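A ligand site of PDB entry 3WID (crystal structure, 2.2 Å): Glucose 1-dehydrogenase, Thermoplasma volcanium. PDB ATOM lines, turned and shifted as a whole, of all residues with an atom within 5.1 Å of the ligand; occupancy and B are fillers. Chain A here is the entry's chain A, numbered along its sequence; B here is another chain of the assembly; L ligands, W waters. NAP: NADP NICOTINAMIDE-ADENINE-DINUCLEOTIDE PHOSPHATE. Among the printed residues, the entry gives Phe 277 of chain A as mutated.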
ATOM      1  N   CYS A  41      24.536   1.698 -33.759  1.00  0.00           N
ATOM      2  CA  CYS A  41      25.063   1.829 -32.388  1.00  0.00           C
ATOM      3  C   CYS A  41      26.393   2.534 -32.534  1.00  0.00           C
ATOM      4  O   CYS A  41      26.821   2.856 -33.642  1.00  0.00           O
ATOM      5  CB  CYS A  41      25.209   0.430 -31.692  1.00  0.00           C
ATOM      6  SG  CYS A  41      26.604  -0.639 -32.166  1.00  0.00           S
ATOM      7  N   GLY A  42      27.086   2.704 -31.414  1.00  0.00           N
ATOM      8  CA  GLY A  42      28.366   3.412 -31.409  1.00  0.00           C
ATOM      9  C   GLY A  42      29.449   2.693 -32.209  1.00  0.00           C
ATOM     10  O   GLY A  42      30.405   3.333 -32.671  1.00  0.00           O
ATOM     11  N   THR A  43      29.334   1.368 -32.375  1.00  0.00           N
ATOM     12  CA  THR A  43      30.317   0.646 -33.188  1.00  0.00           C
ATOM     13  C   THR A  43      30.198   1.052 -34.684  1.00  0.00           C
ATOM     14  O   THR A  43      31.181   1.218 -35.387  1.00  0.00           O
ATOM     15  CB  THR A  43      30.155  -0.869 -32.980  1.00  0.00           C
ATOM     16  OG1 THR A  43      30.272  -1.157 -31.596  1.00  0.00           O
ATOM     17  CG2 THR A  43      31.214  -1.699 -33.749  1.00  0.00           C
ATOM     18  N   ASN A 160      22.754  -9.022 -26.247  1.00  0.00           N
ATOM     19  CA  ASN A 160      23.950  -8.821 -25.456  1.00  0.00           C
ATOM     20  C   ASN A 160      23.641  -8.852 -23.968  1.00  0.00           C
ATOM     21  O   ASN A 160      24.436  -9.326 -23.126  1.00  0.00           O
ATOM     22  CB  ASN A 160      24.534  -7.520 -25.873  1.00  0.00           C
ATOM     23  CG  ASN A 160      25.045  -7.568 -27.319  1.00  0.00           C
ATOM     24  OD1 ASN A 160      25.528  -8.594 -27.777  1.00  0.00           O
ATOM     25  ND2 ASN A 160      24.948  -6.455 -28.031  1.00  0.00           N
ATOM     26  N   ILE A 192      25.424   1.861 -15.051  1.00  0.00           N
ATOM     27  CA  ILE A 192      26.065   3.089 -15.361  1.00  0.00           C
ATOM     28  C   ILE A 192      25.667   3.389 -16.824  1.00  0.00           C
ATOM     29  O   ILE A 192      25.893   2.565 -17.733  1.00  0.00           O
ATOM     30  CB  ILE A 192      27.570   2.958 -15.234  1.00  0.00           C
ATOM     31  CG1 ILE A 192      28.003   2.542 -13.823  1.00  0.00           C
ATOM     32  CG2 ILE A 192      28.225   4.272 -15.583  1.00  0.00           C
ATOM     33  CD1 ILE A 192      29.463   2.067 -13.833  1.00  0.00           C
ATOM     34  N   GLY A 193      25.159   4.585 -17.058  1.00  0.00           N
ATOM     35  CA  GLY A 193      24.670   5.002 -18.350  1.00  0.00           C
ATOM     36  C   GLY A 193      23.165   5.044 -18.451  1.00  0.00           C
ATOM     37  O   GLY A 193      22.486   4.496 -17.635  1.00  0.00           O
ATOM     38  N   SER A 194      22.670   5.764 -19.441  1.00  0.00           N
ATOM     39  CA  SER A 194      21.240   5.867 -19.673  1.00  0.00           C
ATOM     40  C   SER A 194      20.857   5.808 -21.153  1.00  0.00           C
ATOM     41  O   SER A 194      19.869   6.360 -21.555  1.00  0.00           O
ATOM     42  CB  SER A 194      20.619   7.068 -18.948  1.00  0.00           C
ATOM     43  OG  SER A 194      21.305   8.257 -19.172  1.00  0.00           O
ATOM     44  N   GLY A 195      21.695   5.150 -21.935  1.00  0.00           N
ATOM     45  CA  GLY A 195      21.468   4.902 -23.342  1.00  0.00           C
ATOM     46  C   GLY A 195      20.670   3.644 -23.578  1.00  0.00           C
ATOM     47  O   GLY A 195      20.157   3.080 -22.673  1.00  0.00           O
ATOM     48  N   SER A 196      20.527   3.236 -24.822  1.00  0.00           N
ATOM     49  CA  SER A 196      19.681   2.148 -25.149  1.00  0.00           C
ATOM     50  C   SER A 196      20.151   0.818 -24.458  1.00  0.00           C
ATOM     51  O   SER A 196      19.334   0.095 -23.936  1.00  0.00           O
ATOM     52  CB  SER A 196      19.580   2.010 -26.662  1.00  0.00           C
ATOM     53  OG  SER A 196      20.822   1.648 -27.191  1.00  0.00           O
ATOM     54  N   GLU A 197      21.410   0.518 -24.459  1.00  0.00           N
ATOM     55  CA  GLU A 197      21.897  -0.681 -23.773  1.00  0.00           C
ATOM     56  C   GLU A 197      21.543  -0.631 -22.259  1.00  0.00           C
ATOM     57  O   GLU A 197      20.942  -1.612 -21.676  1.00  0.00           O
ATOM     58  CB  GLU A 197      23.397  -0.898 -24.011  1.00  0.00           C
ATOM     59  CG  GLU A 197      23.820  -1.389 -25.432  1.00  0.00           C
ATOM     60  CD  GLU A 197      23.440  -2.893 -25.697  1.00  0.00           C
ATOM     61  OE1 GLU A 197      24.157  -3.632 -26.447  1.00  0.00           O
ATOM     62  OE2 GLU A 197      22.374  -3.347 -25.204  1.00  0.00           O
ATOM     63  N   ALA A 198      21.784   0.519 -21.658  1.00  0.00           N
ATOM     64  CA  ALA A 198      21.419   0.680 -20.229  1.00  0.00           C
ATOM     65  C   ALA A 198      19.935   0.500 -19.987  1.00  0.00           C
ATOM     66  O   ALA A 198      19.496  -0.156 -18.990  1.00  0.00           O
ATOM     67  CB  ALA A 198      21.938   2.013 -19.705  1.00  0.00           C
ATOM     68  N   VAL A 215      22.181   5.458 -13.981  1.00  0.00           N
ATOM     69  CA  VAL A 215      22.827   6.605 -13.511  1.00  0.00           C
ATOM     70  C   VAL A 215      23.676   7.195 -14.593  1.00  0.00           C
ATOM     71  O   VAL A 215      24.200   6.499 -15.457  1.00  0.00           O
ATOM     72  CB  VAL A 215      23.680   6.327 -12.266  1.00  0.00           C
ATOM     73  CG1 VAL A 215      22.784   5.766 -11.162  1.00  0.00           C
ATOM     74  CG2 VAL A 215      24.892   5.438 -12.576  1.00  0.00           C
ATOM     75  N   ASN A 216      23.808   8.519 -14.519  1.00  0.00           N
ATOM     76  CA  ASN A 216      24.685   9.268 -15.417  1.00  0.00           C
ATOM     77  C   ASN A 216      25.218  10.515 -14.696  1.00  0.00           C
ATOM     78  O   ASN A 216      24.697  10.899 -13.611  1.00  0.00           O
ATOM     79  CB  ASN A 216      23.920   9.682 -16.676  1.00  0.00           C
ATOM     80  CG  ASN A 216      24.754   9.616 -17.928  1.00  0.00           C
ATOM     81  OD1 ASN A 216      25.922  10.031 -17.934  1.00  0.00           O
ATOM     82  ND2 ASN A 216      24.179   9.057 -18.975  1.00  0.00           N
ATOM     83  N   ARG A 217      26.219  11.159 -15.325  1.00  0.00           N
ATOM     84  CA  ARG A 217      26.888  12.362 -14.785  1.00  0.00           C
ATOM     85  C   ARG A 217      26.188  13.689 -15.160  1.00  0.00           C
ATOM     86  O   ARG A 217      26.813  14.749 -15.202  1.00  0.00           O
ATOM     87  CB  ARG A 217      28.366  12.402 -15.222  1.00  0.00           C
ATOM     88  CG  ARG A 217      28.591  12.635 -16.715  1.00  0.00           C
ATOM     89  CD  ARG A 217      29.809  11.853 -17.143  1.00  0.00           C
ATOM     90  NE  ARG A 217      30.128  11.832 -18.579  1.00  0.00           N
ATOM     91  CZ  ARG A 217      29.296  11.502 -19.599  1.00  0.00           C
ATOM     92  NH1 ARG A 217      29.779  11.479 -20.839  1.00  0.00           N
ATOM     93  NH2 ARG A 217      27.999  11.262 -19.429  1.00  0.00           N
ATOM     94  N   HIS A 218      24.893  13.625 -15.388  1.00  0.00           N
ATOM     95  CA  HIS A 218      24.091  14.757 -15.818  1.00  0.00           C
ATOM     96  C   HIS A 218      22.661  14.289 -15.741  1.00  0.00           C
ATOM     97  O   HIS A 218      22.396  13.083 -15.768  1.00  0.00           O
ATOM     98  CB  HIS A 218      24.458  15.196 -17.264  1.00  0.00           C
ATOM     99  CG  HIS A 218      24.133  14.202 -18.337  1.00  0.00           C
ATOM    100  ND1 HIS A 218      22.842  13.822 -18.652  1.00  0.00           N
ATOM    101  CD2 HIS A 218      24.931  13.536 -19.214  1.00  0.00           C
ATOM    102  CE1 HIS A 218      22.856  12.962 -19.652  1.00  0.00           C
ATOM    103  NE2 HIS A 218      24.117  12.779 -20.018  1.00  0.00           N
ATOM    104  N   TYR A 238      24.570  11.035 -10.678  1.00  0.00           N
ATOM    105  CA  TYR A 238      25.353  10.535  -9.544  1.00  0.00           C
ATOM    106  C   TYR A 238      26.220  11.598  -8.916  1.00  0.00           C
ATOM    107  O   TYR A 238      26.616  11.454  -7.760  1.00  0.00           O
ATOM    108  CB  TYR A 238      26.181   9.247  -9.867  1.00  0.00           C
ATOM    109  CG  TYR A 238      27.173   9.322 -11.014  1.00  0.00           C
ATOM    110  CD1 TYR A 238      28.324  10.093 -10.943  1.00  0.00           C
ATOM    111  CD2 TYR A 238      26.955   8.577 -12.155  1.00  0.00           C
ATOM    112  CE1 TYR A 238      29.208  10.123 -11.989  1.00  0.00           C
ATOM    113  CE2 TYR A 238      27.831   8.616 -13.193  1.00  0.00           C
ATOM    114  CZ  TYR A 238      28.950   9.373 -13.112  1.00  0.00           C
ATOM    115  OH  TYR A 238      29.786   9.350 -14.204  1.00  0.00           O
ATOM    116  N   THR A 252      27.845   0.489 -18.888  1.00  0.00           N
ATOM    117  CA  THR A 252      27.746   0.747 -20.325  1.00  0.00           C
ATOM    118  C   THR A 252      28.584   1.923 -20.793  1.00  0.00           C
ATOM    119  O   THR A 252      28.549   2.227 -21.985  1.00  0.00           O
ATOM    120  CB  THR A 252      26.296   0.968 -20.749  1.00  0.00           C
ATOM    121  OG1 THR A 252      25.878   2.286 -20.391  1.00  0.00           O
ATOM    122  CG2 THR A 252      25.394  -0.009 -20.101  1.00  0.00           C
ATOM    123  N   SER A 253      29.362   2.540 -19.908  1.00  0.00           N
ATOM    124  CA  SER A 253      30.211   3.738 -20.263  1.00  0.00           C
ATOM    125  C   SER A 253      31.550   3.397 -20.902  1.00  0.00           C
ATOM    126  O   SER A 253      31.975   3.986 -21.873  1.00  0.00           O
ATOM    127  CB  SER A 253      30.460   4.570 -19.013  1.00  0.00           C
ATOM    128  OG  SER A 253      31.373   3.913 -18.122  1.00  0.00           O
ATOM    129  N   ASP A 255      34.103   3.674 -19.113  1.00  0.00           N
ATOM    130  CA  ASP A 255      34.975   4.653 -18.426  1.00  0.00           C
ATOM    131  C   ASP A 255      35.470   4.175 -17.078  1.00  0.00           C
ATOM    132  O   ASP A 255      34.664   3.996 -16.161  1.00  0.00           O
ATOM    133  CB  ASP A 255      34.232   5.962 -18.202  1.00  0.00           C
ATOM    134  CG  ASP A 255      35.120   6.995 -17.581  1.00  0.00           C
ATOM    135  OD1 ASP A 255      36.182   7.306 -18.165  1.00  0.00           O
ATOM    136  OD2 ASP A 255      34.746   7.478 -16.493  1.00  0.00           O
ATOM    137  N   THR A 258      34.640   6.010 -13.648  1.00  0.00           N
ATOM    138  CA  THR A 258      33.262   5.760 -13.248  1.00  0.00           C
ATOM    139  C   THR A 258      33.113   4.275 -12.805  1.00  0.00           C
ATOM    140  O   THR A 258      32.479   3.973 -11.797  1.00  0.00           O
ATOM    141  CB  THR A 258      32.307   6.073 -14.403  1.00  0.00           C
ATOM    142  OG1 THR A 258      32.711   7.290 -15.024  1.00  0.00           O
ATOM    143  CG2 THR A 258      30.887   6.165 -13.951  1.00  0.00           C
ATOM    144  N   PHE A 275      30.672  -4.185 -19.701  1.00  0.00           N
ATOM    145  CA  PHE A 275      30.076  -4.361 -20.997  1.00  0.00           C
ATOM    146  C   PHE A 275      30.456  -3.236 -21.944  1.00  0.00           C
ATOM    147  O   PHE A 275      30.718  -3.455 -23.093  1.00  0.00           O
ATOM    148  CB  PHE A 275      28.566  -4.531 -20.829  1.00  0.00           C
ATOM    149  CG  PHE A 275      27.818  -4.615 -22.096  1.00  0.00           C
ATOM    150  CD1 PHE A 275      27.658  -5.804 -22.750  1.00  0.00           C
ATOM    151  CD2 PHE A 275      27.273  -3.489 -22.656  1.00  0.00           C
ATOM    152  CE1 PHE A 275      26.995  -5.866 -23.944  1.00  0.00           C
ATOM    153  CE2 PHE A 275      26.597  -3.545 -23.830  1.00  0.00           C
ATOM    154  CZ  PHE A 275      26.456  -4.742 -24.480  1.00  0.00           C
ATOM    155  N   GLY A 276      30.478  -2.021 -21.445  1.00  0.00           N
ATOM    156  CA  GLY A 276      30.842  -0.895 -22.254  1.00  0.00           C
ATOM    157  C   GLY A 276      32.309  -0.876 -22.564  1.00  0.00           C
ATOM    158  O   GLY A 276      33.107  -1.355 -21.811  1.00  0.00           O
ATOM    159  N   PHE A 277      32.670  -0.321 -23.695  1.00  0.00           N
ATOM    160  CA  PHE A 277      34.051  -0.003 -23.938  1.00  0.00           C
ATOM    161  C   PHE A 277      34.260   1.254 -24.786  1.00  0.00           C
ATOM    162  O   PHE A 277      33.489   1.586 -25.689  1.00  0.00           O
ATOM    163  CB  PHE A 277      34.800  -1.202 -24.512  1.00  0.00           C
ATOM    164  CG  PHE A 277      34.355  -1.614 -25.881  1.00  0.00           C
ATOM    165  CD1 PHE A 277      34.831  -0.955 -27.010  1.00  0.00           C
ATOM    166  CD2 PHE A 277      33.494  -2.692 -26.053  1.00  0.00           C
ATOM    167  CE1 PHE A 277      34.451  -1.349 -28.267  1.00  0.00           C
ATOM    168  CE2 PHE A 277      33.092  -3.081 -27.300  1.00  0.00           C
ATOM    169  CZ  PHE A 277      33.574  -2.405 -28.416  1.00  0.00           C
ATOM    170  N   ASN A 278      35.351   1.937 -24.443  1.00  0.00           N
ATOM    171  CA  ASN A 278      35.785   3.134 -25.090  1.00  0.00           C
ATOM    172  C   ASN A 278      37.309   3.236 -24.968  1.00  0.00           C
ATOM    173  O   ASN A 278      37.843   3.573 -23.897  1.00  0.00           O
ATOM    174  CB  ASN A 278      35.129   4.330 -24.429  1.00  0.00           C
ATOM    175  CG  ASN A 278      35.655   5.634 -25.004  1.00  0.00           C
ATOM    176  OD1 ASN A 278      36.263   5.654 -26.093  1.00  0.00           O
ATOM    177  ND2 ASN A 278      35.444   6.713 -24.262  1.00  0.00           N
ATOM    178  N   SER A 304      31.824  -9.215 -20.575  1.00  0.00           N
ATOM    179  CA  SER A 304      30.871  -9.941 -21.398  1.00  0.00           C
ATOM    180  C   SER A 304      30.777  -9.337 -22.777  1.00  0.00           C
ATOM    181  O   SER A 304      30.481  -8.173 -22.905  1.00  0.00           O
ATOM    182  CB  SER A 304      29.515  -9.889 -20.733  1.00  0.00           C
ATOM    183  OG  SER A 304      28.577 -10.692 -21.410  1.00  0.00           O
ATOM    184  N   VAL A 305      30.956 -10.128 -23.828  1.00  0.00           N
ATOM    185  CA  VAL A 305      30.761  -9.639 -25.193  1.00  0.00           C
ATOM    186  C   VAL A 305      29.818 -10.566 -25.972  1.00  0.00           C
ATOM    187  O   VAL A 305      29.916 -11.812 -25.888  1.00  0.00           O
ATOM    188  CB  VAL A 305      32.078  -9.492 -25.932  1.00  0.00           C
ATOM    189  CG1 VAL A 305      32.740 -10.847 -26.137  1.00  0.00           C
ATOM    190  CG2 VAL A 305      31.875  -8.797 -27.286  1.00  0.00           C
ATOM    191  N   ASP A 306      28.907  -9.946 -26.727  1.00  0.00           N
ATOM    192  CA  ASP A 306      28.078 -10.633 -27.754  1.00  0.00           C
ATOM    193  C   ASP A 306      27.173 -11.646 -27.062  1.00  0.00           C
ATOM    194  O   ASP A 306      26.933 -11.545 -25.849  1.00  0.00           O
ATOM    195  CB  ASP A 306      28.988 -11.287 -28.784  1.00  0.00           C
ATOM    196  CG  ASP A 306      28.414 -11.293 -30.188  1.00  0.00           C
ATOM    197  OD1 ASP A 306      27.229 -11.631 -30.374  1.00  0.00           O
ATOM    198  OD2 ASP A 306      29.190 -10.997 -31.134  1.00  0.00           O
ATOM    199  N   LYS A 349      24.505  12.555 -34.059  1.00  0.00           N
ATOM    200  CA  LYS A 349      23.465  11.833 -33.360  1.00  0.00           C
ATOM    201  C   LYS A 349      22.237  12.690 -33.399  1.00  0.00           C
ATOM    202  O   LYS A 349      22.289  13.832 -33.057  1.00  0.00           O
ATOM    203  CB  LYS A 349      23.860  11.568 -31.906  1.00  0.00           C
ATOM    204  CG  LYS A 349      25.307  11.134 -31.753  1.00  0.00           C
ATOM    205  CD  LYS A 349      25.757  11.225 -30.308  1.00  0.00           C
ATOM    206  CE  LYS A 349      25.303  10.016 -29.526  1.00  0.00           C
ATOM    207  NZ  LYS A 349      26.390   9.600 -28.611  1.00  0.00           N
ATOM    208  N   LYS A 355      17.493   4.981 -29.600  1.00  0.00           N
ATOM    209  CA  LYS A 355      17.881   4.125 -30.732  1.00  0.00           C
ATOM    210  C   LYS A 355      17.450   4.685 -32.097  1.00  0.00           C
ATOM    211  O   LYS A 355      16.248   4.787 -32.414  1.00  0.00           O
ATOM    212  CB  LYS A 355      17.291   2.702 -30.522  1.00  0.00           C
ATOM    213  CG  LYS A 355      17.523   1.741 -31.676  1.00  0.00           C
ATOM    214  CD  LYS A 355      18.998   1.607 -31.993  1.00  0.00           C
ATOM    215  CE  LYS A 355      19.706   0.870 -30.870  1.00  0.00           C
ATOM    216  NZ  LYS A 355      21.157   0.678 -31.199  1.00  0.00           N
ATOM    217  N   VAL B 295      36.611  -7.026 -21.618  1.00  0.00           N
ATOM    218  CA  VAL B 295      35.291  -7.237 -22.199  1.00  0.00           C
ATOM    219  C   VAL B 295      35.337  -8.128 -23.436  1.00  0.00           C
ATOM    220  O   VAL B 295      34.651  -9.156 -23.465  1.00  0.00           O
ATOM    221  CB  VAL B 295      34.594  -5.910 -22.528  1.00  0.00           C
ATOM    222  CG1 VAL B 295      33.267  -6.102 -23.256  1.00  0.00           C
ATOM    223  CG2 VAL B 295      34.418  -5.159 -21.236  1.00  0.00           C
HETATM  224  PA  NAP L   1      25.387   4.655 -25.839  1.00  0.00           P
HETATM  225  O1A NAP L   1      23.950   4.862 -26.014  1.00  0.00           O
HETATM  226  O2A NAP L   1      26.316   5.673 -26.351  1.00  0.00           O
HETATM  227  O5B NAP L   1      25.615   4.458 -24.284  1.00  0.00           O
HETATM  228  C5B NAP L   1      26.671   5.049 -23.565  1.00  0.00           C
HETATM  229  C4B NAP L   1      26.048   5.599 -22.301  1.00  0.00           C
HETATM  230  O4B NAP L   1      27.056   5.843 -21.361  1.00  0.00           O
HETATM  231  C3B NAP L   1      25.396   6.937 -22.548  1.00  0.00           C
HETATM  232  O3B NAP L   1      24.249   6.965 -21.746  1.00  0.00           O
HETATM  233  C2B NAP L   1      26.399   7.933 -22.030  1.00  0.00           C
HETATM  234  O2B NAP L   1      25.802   9.201 -21.735  1.00  0.00           O
HETATM  235  C1B NAP L   1      26.925   7.145 -20.842  1.00  0.00           C
HETATM  236  N9A NAP L   1      28.206   7.582 -20.271  1.00  0.00           N
HETATM  237  C8A NAP L   1      29.331   7.886 -20.912  1.00  0.00           C
HETATM  238  N7A NAP L   1      30.272   8.243 -20.042  1.00  0.00           N
HETATM  239  C5A NAP L   1      29.744   8.159 -18.831  1.00  0.00           C
HETATM  240  C6A NAP L   1      30.184   8.385 -17.472  1.00  0.00           C
HETATM  241  N6A NAP L   1      31.437   8.797 -17.229  1.00  0.00           N
HETATM  242  N1A NAP L   1      29.327   8.192 -16.498  1.00  0.00           N
HETATM  243  C2A NAP L   1      28.093   7.783 -16.720  1.00  0.00           C
HETATM  244  N3A NAP L   1      27.634   7.550 -17.936  1.00  0.00           N
HETATM  245  C4A NAP L   1      28.387   7.725 -18.996  1.00  0.00           C
HETATM  246  O3  NAP L   1      25.730   3.222 -26.437  1.00  0.00           O
HETATM  247  PN  NAP L   1      24.922   1.879 -26.176  1.00  0.00           P
HETATM  248  O1N NAP L   1      24.486   1.390 -27.490  1.00  0.00           O
HETATM  249  O2N NAP L   1      23.918   2.034 -25.111  1.00  0.00           O
HETATM  250  O5D NAP L   1      26.072   0.897 -25.682  1.00  0.00           O
HETATM  251  C5D NAP L   1      26.899   1.182 -24.567  1.00  0.00           C
HETATM  252  C4D NAP L   1      28.325   0.647 -24.667  1.00  0.00           C
HETATM  253  O4D NAP L   1      28.387  -0.749 -24.932  1.00  0.00           O
HETATM  254  C3D NAP L   1      29.196   1.296 -25.714  1.00  0.00           C
HETATM  255  O3D NAP L   1      30.397   1.639 -25.073  1.00  0.00           O
HETATM  256  C2D NAP L   1      29.560   0.213 -26.683  1.00  0.00           C
HETATM  257  O2D NAP L   1      30.914   0.413 -27.018  1.00  0.00           O
HETATM  258  C1D NAP L   1      29.393  -1.041 -25.874  1.00  0.00           C
HETATM  259  N1N NAP L   1      28.974  -2.223 -26.616  1.00  0.00           N
HETATM  260  C2N NAP L   1      29.265  -3.398 -26.079  1.00  0.00           C
HETATM  261  C3N NAP L   1      28.912  -4.574 -26.680  1.00  0.00           C
HETATM  262  C7N NAP L   1      29.247  -5.891 -26.078  1.00  0.00           C
HETATM  263  O7N NAP L   1      28.723  -6.874 -26.546  1.00  0.00           O
HETATM  264  N7N NAP L   1      30.076  -5.981 -25.063  1.00  0.00           N
HETATM  265  C4N NAP L   1      28.217  -4.507 -27.864  1.00  0.00           C
HETATM  266  C5N NAP L   1      27.919  -3.269 -28.390  1.00  0.00           C
HETATM  267  C6N NAP L   1      28.309  -2.120 -27.753  1.00  0.00           C
HETATM  268  P2B NAP L   1      25.947  10.471 -22.689  1.00  0.00           P
HETATM  269  O1X NAP L   1      25.498  10.022 -24.014  1.00  0.00           O
HETATM  270  O2X NAP L   1      25.099  11.452 -22.008  1.00  0.00           O
HETATM  271  O3X NAP L   1      27.342  10.901 -22.732  1.00  0.00           O
HETATM  272  O   HOH W   1      22.604  -0.332 -28.630  1.00  0.00           O
HETATM  273  O   HOH W   2      23.624   3.036 -30.171  1.00  0.00           O
HETATM  274  O   HOH W   3      23.647   2.585 -22.343  1.00  0.00           O
HETATM  275  O   HOH W   4      26.861   1.474 -28.764  1.00  0.00           O
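Asn 160 touches the ligand.
CG2 of Ile 192 touches C2A of the ligand (3.7 Å).
CA of Gly 193 touches N3A of the ligand (3.9 Å).
Ser 196 touches the ligand (N to O2N, 3.6 Å).
Thr 252 touches the ligand.
CB of Ser 253 touches C5A of the ligand, at 3.7 Å.
OD2 of Asp 255 touches N6A of the ligand, at 3.6 Å.
Gly 276 touches the ligand.
Val 305 touches the ligand.
Val 295 of chain B touches the ligand.
Hydrophobic or aromatic side chains that line the ligand: Ile 192, His 218, Tyr 238, Phe 275, Val 305 and Val 295 of chain B.
22 residues have an atom within 4 Å of the ligand: Asn 160, Ile 192, Gly 193, Ser 194, Gly 195, Ser 196, Glu 197, Asn 216, Arg 217, His 218, Tyr 238, Thr 252, Ser 253, Asp 255, Thr 258, Phe 275, Gly 276, Phe 277, Ser 304, Val 305, Asp 306 and Val 295 of chain B.
The nearest printed residue that does not touch the ligand is Val 215 (4.3 Å).
O of Phe 277 sits at hydrogen-bond distance from O2D of the ligand, 3.1 Å away.
A nitrogen (N3A) of the ligand lies close to the side-chain amide oxygen (OD1) of Asn 216.
OH of Tyr 238 is in hydrogen-bond range of N1A of the ligand (2.6 Å).
NH1 of Arg 217 is in salt-bridge range of O3X of the ligand.
The backbone NH (N) of Gly 195 is in hydrogen-bond range of an oxygen (O3B) of the ligand (3.1 Å).
The backbone carbonyl oxygen (O) of Phe 275 sits at hydrogen-bond distance from a nitrogen (N7N) of the ligand (3.3 Å).
An oxygen (O3D) of the ligand lies within hydrogen-bond range of the backbone NH (N) of Phe 277 (3.3 Å).
N7N of the ligand is in hydrogen-bond range of O of Ser 304, at 3.1 Å.
An oxygen (O2X) of the ligand is in hydrogen-bond range of a ring nitrogen (NE2) of His 218 (2.6 Å).
N of Asp 306 sits at hydrogen-bond distance from O7N of the ligand (3.1 Å).
N of Ser 194 sits at hydrogen-bond distance from O3B of the ligand.
A nitrogen (N6A) of the ligand sits at hydrogen-bond distance from the side-chain hydroxyl (OG1) of Thr 258 (3.0 Å).
An oxygen (O2N) of the ligand sits at hydrogen-bond distance from the backbone NH of Glu 197 (3.0 Å).
The side-chain amide oxygen (OD1) of Asn 216 sits at hydrogen-bond distance from the guanidinium group (NH2) of Arg 217, 2.8 Å away.
The backbone carbonyl oxygen (O) of Asn 216 sits at hydrogen-bond distance from the backbone NH (N) of Tyr 238.
The side-chain hydroxyl of Thr 258 sits at hydrogen-bond distance from the side-chain carboxylate of Asp 255 (2.5 Å).
The side-chain amide nitrogen (ND2) of Asn 216 sits at hydrogen-bond distance from the side-chain hydroxyl (OG) of Ser 194, 3.0 Å away.
OG1 of Thr 252 is in hydrogen-bond range of O of Ile 192 (2.7 Å).
O of Val 215 lies within hydrogen-bond range of N of Gly 193, at 2.7 Å.
OG of Ser 253 sits at hydrogen-bond distance from N of Asp 255, at 2.9 Å.
OE1 of Glu 197 sits at hydrogen-bond distance from ND2 of Asn 160, at 3.3 Å.
Water W4 lies within hydrogen-bond range of O1N of the ligand (2.7 Å) and N of Gly 42 (2.9 Å).
Water W1 lies within hydrogen-bond range of O1N of the ligand (2.8 Å), OG of Ser 196 (3.0 Å) and NZ of Lys 355 (3.1 Å).
Water W3 lies within hydrogen-bond range of O2N of the ligand, N of Ala 198, OG1 of Thr 252 and N of Gly 195.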
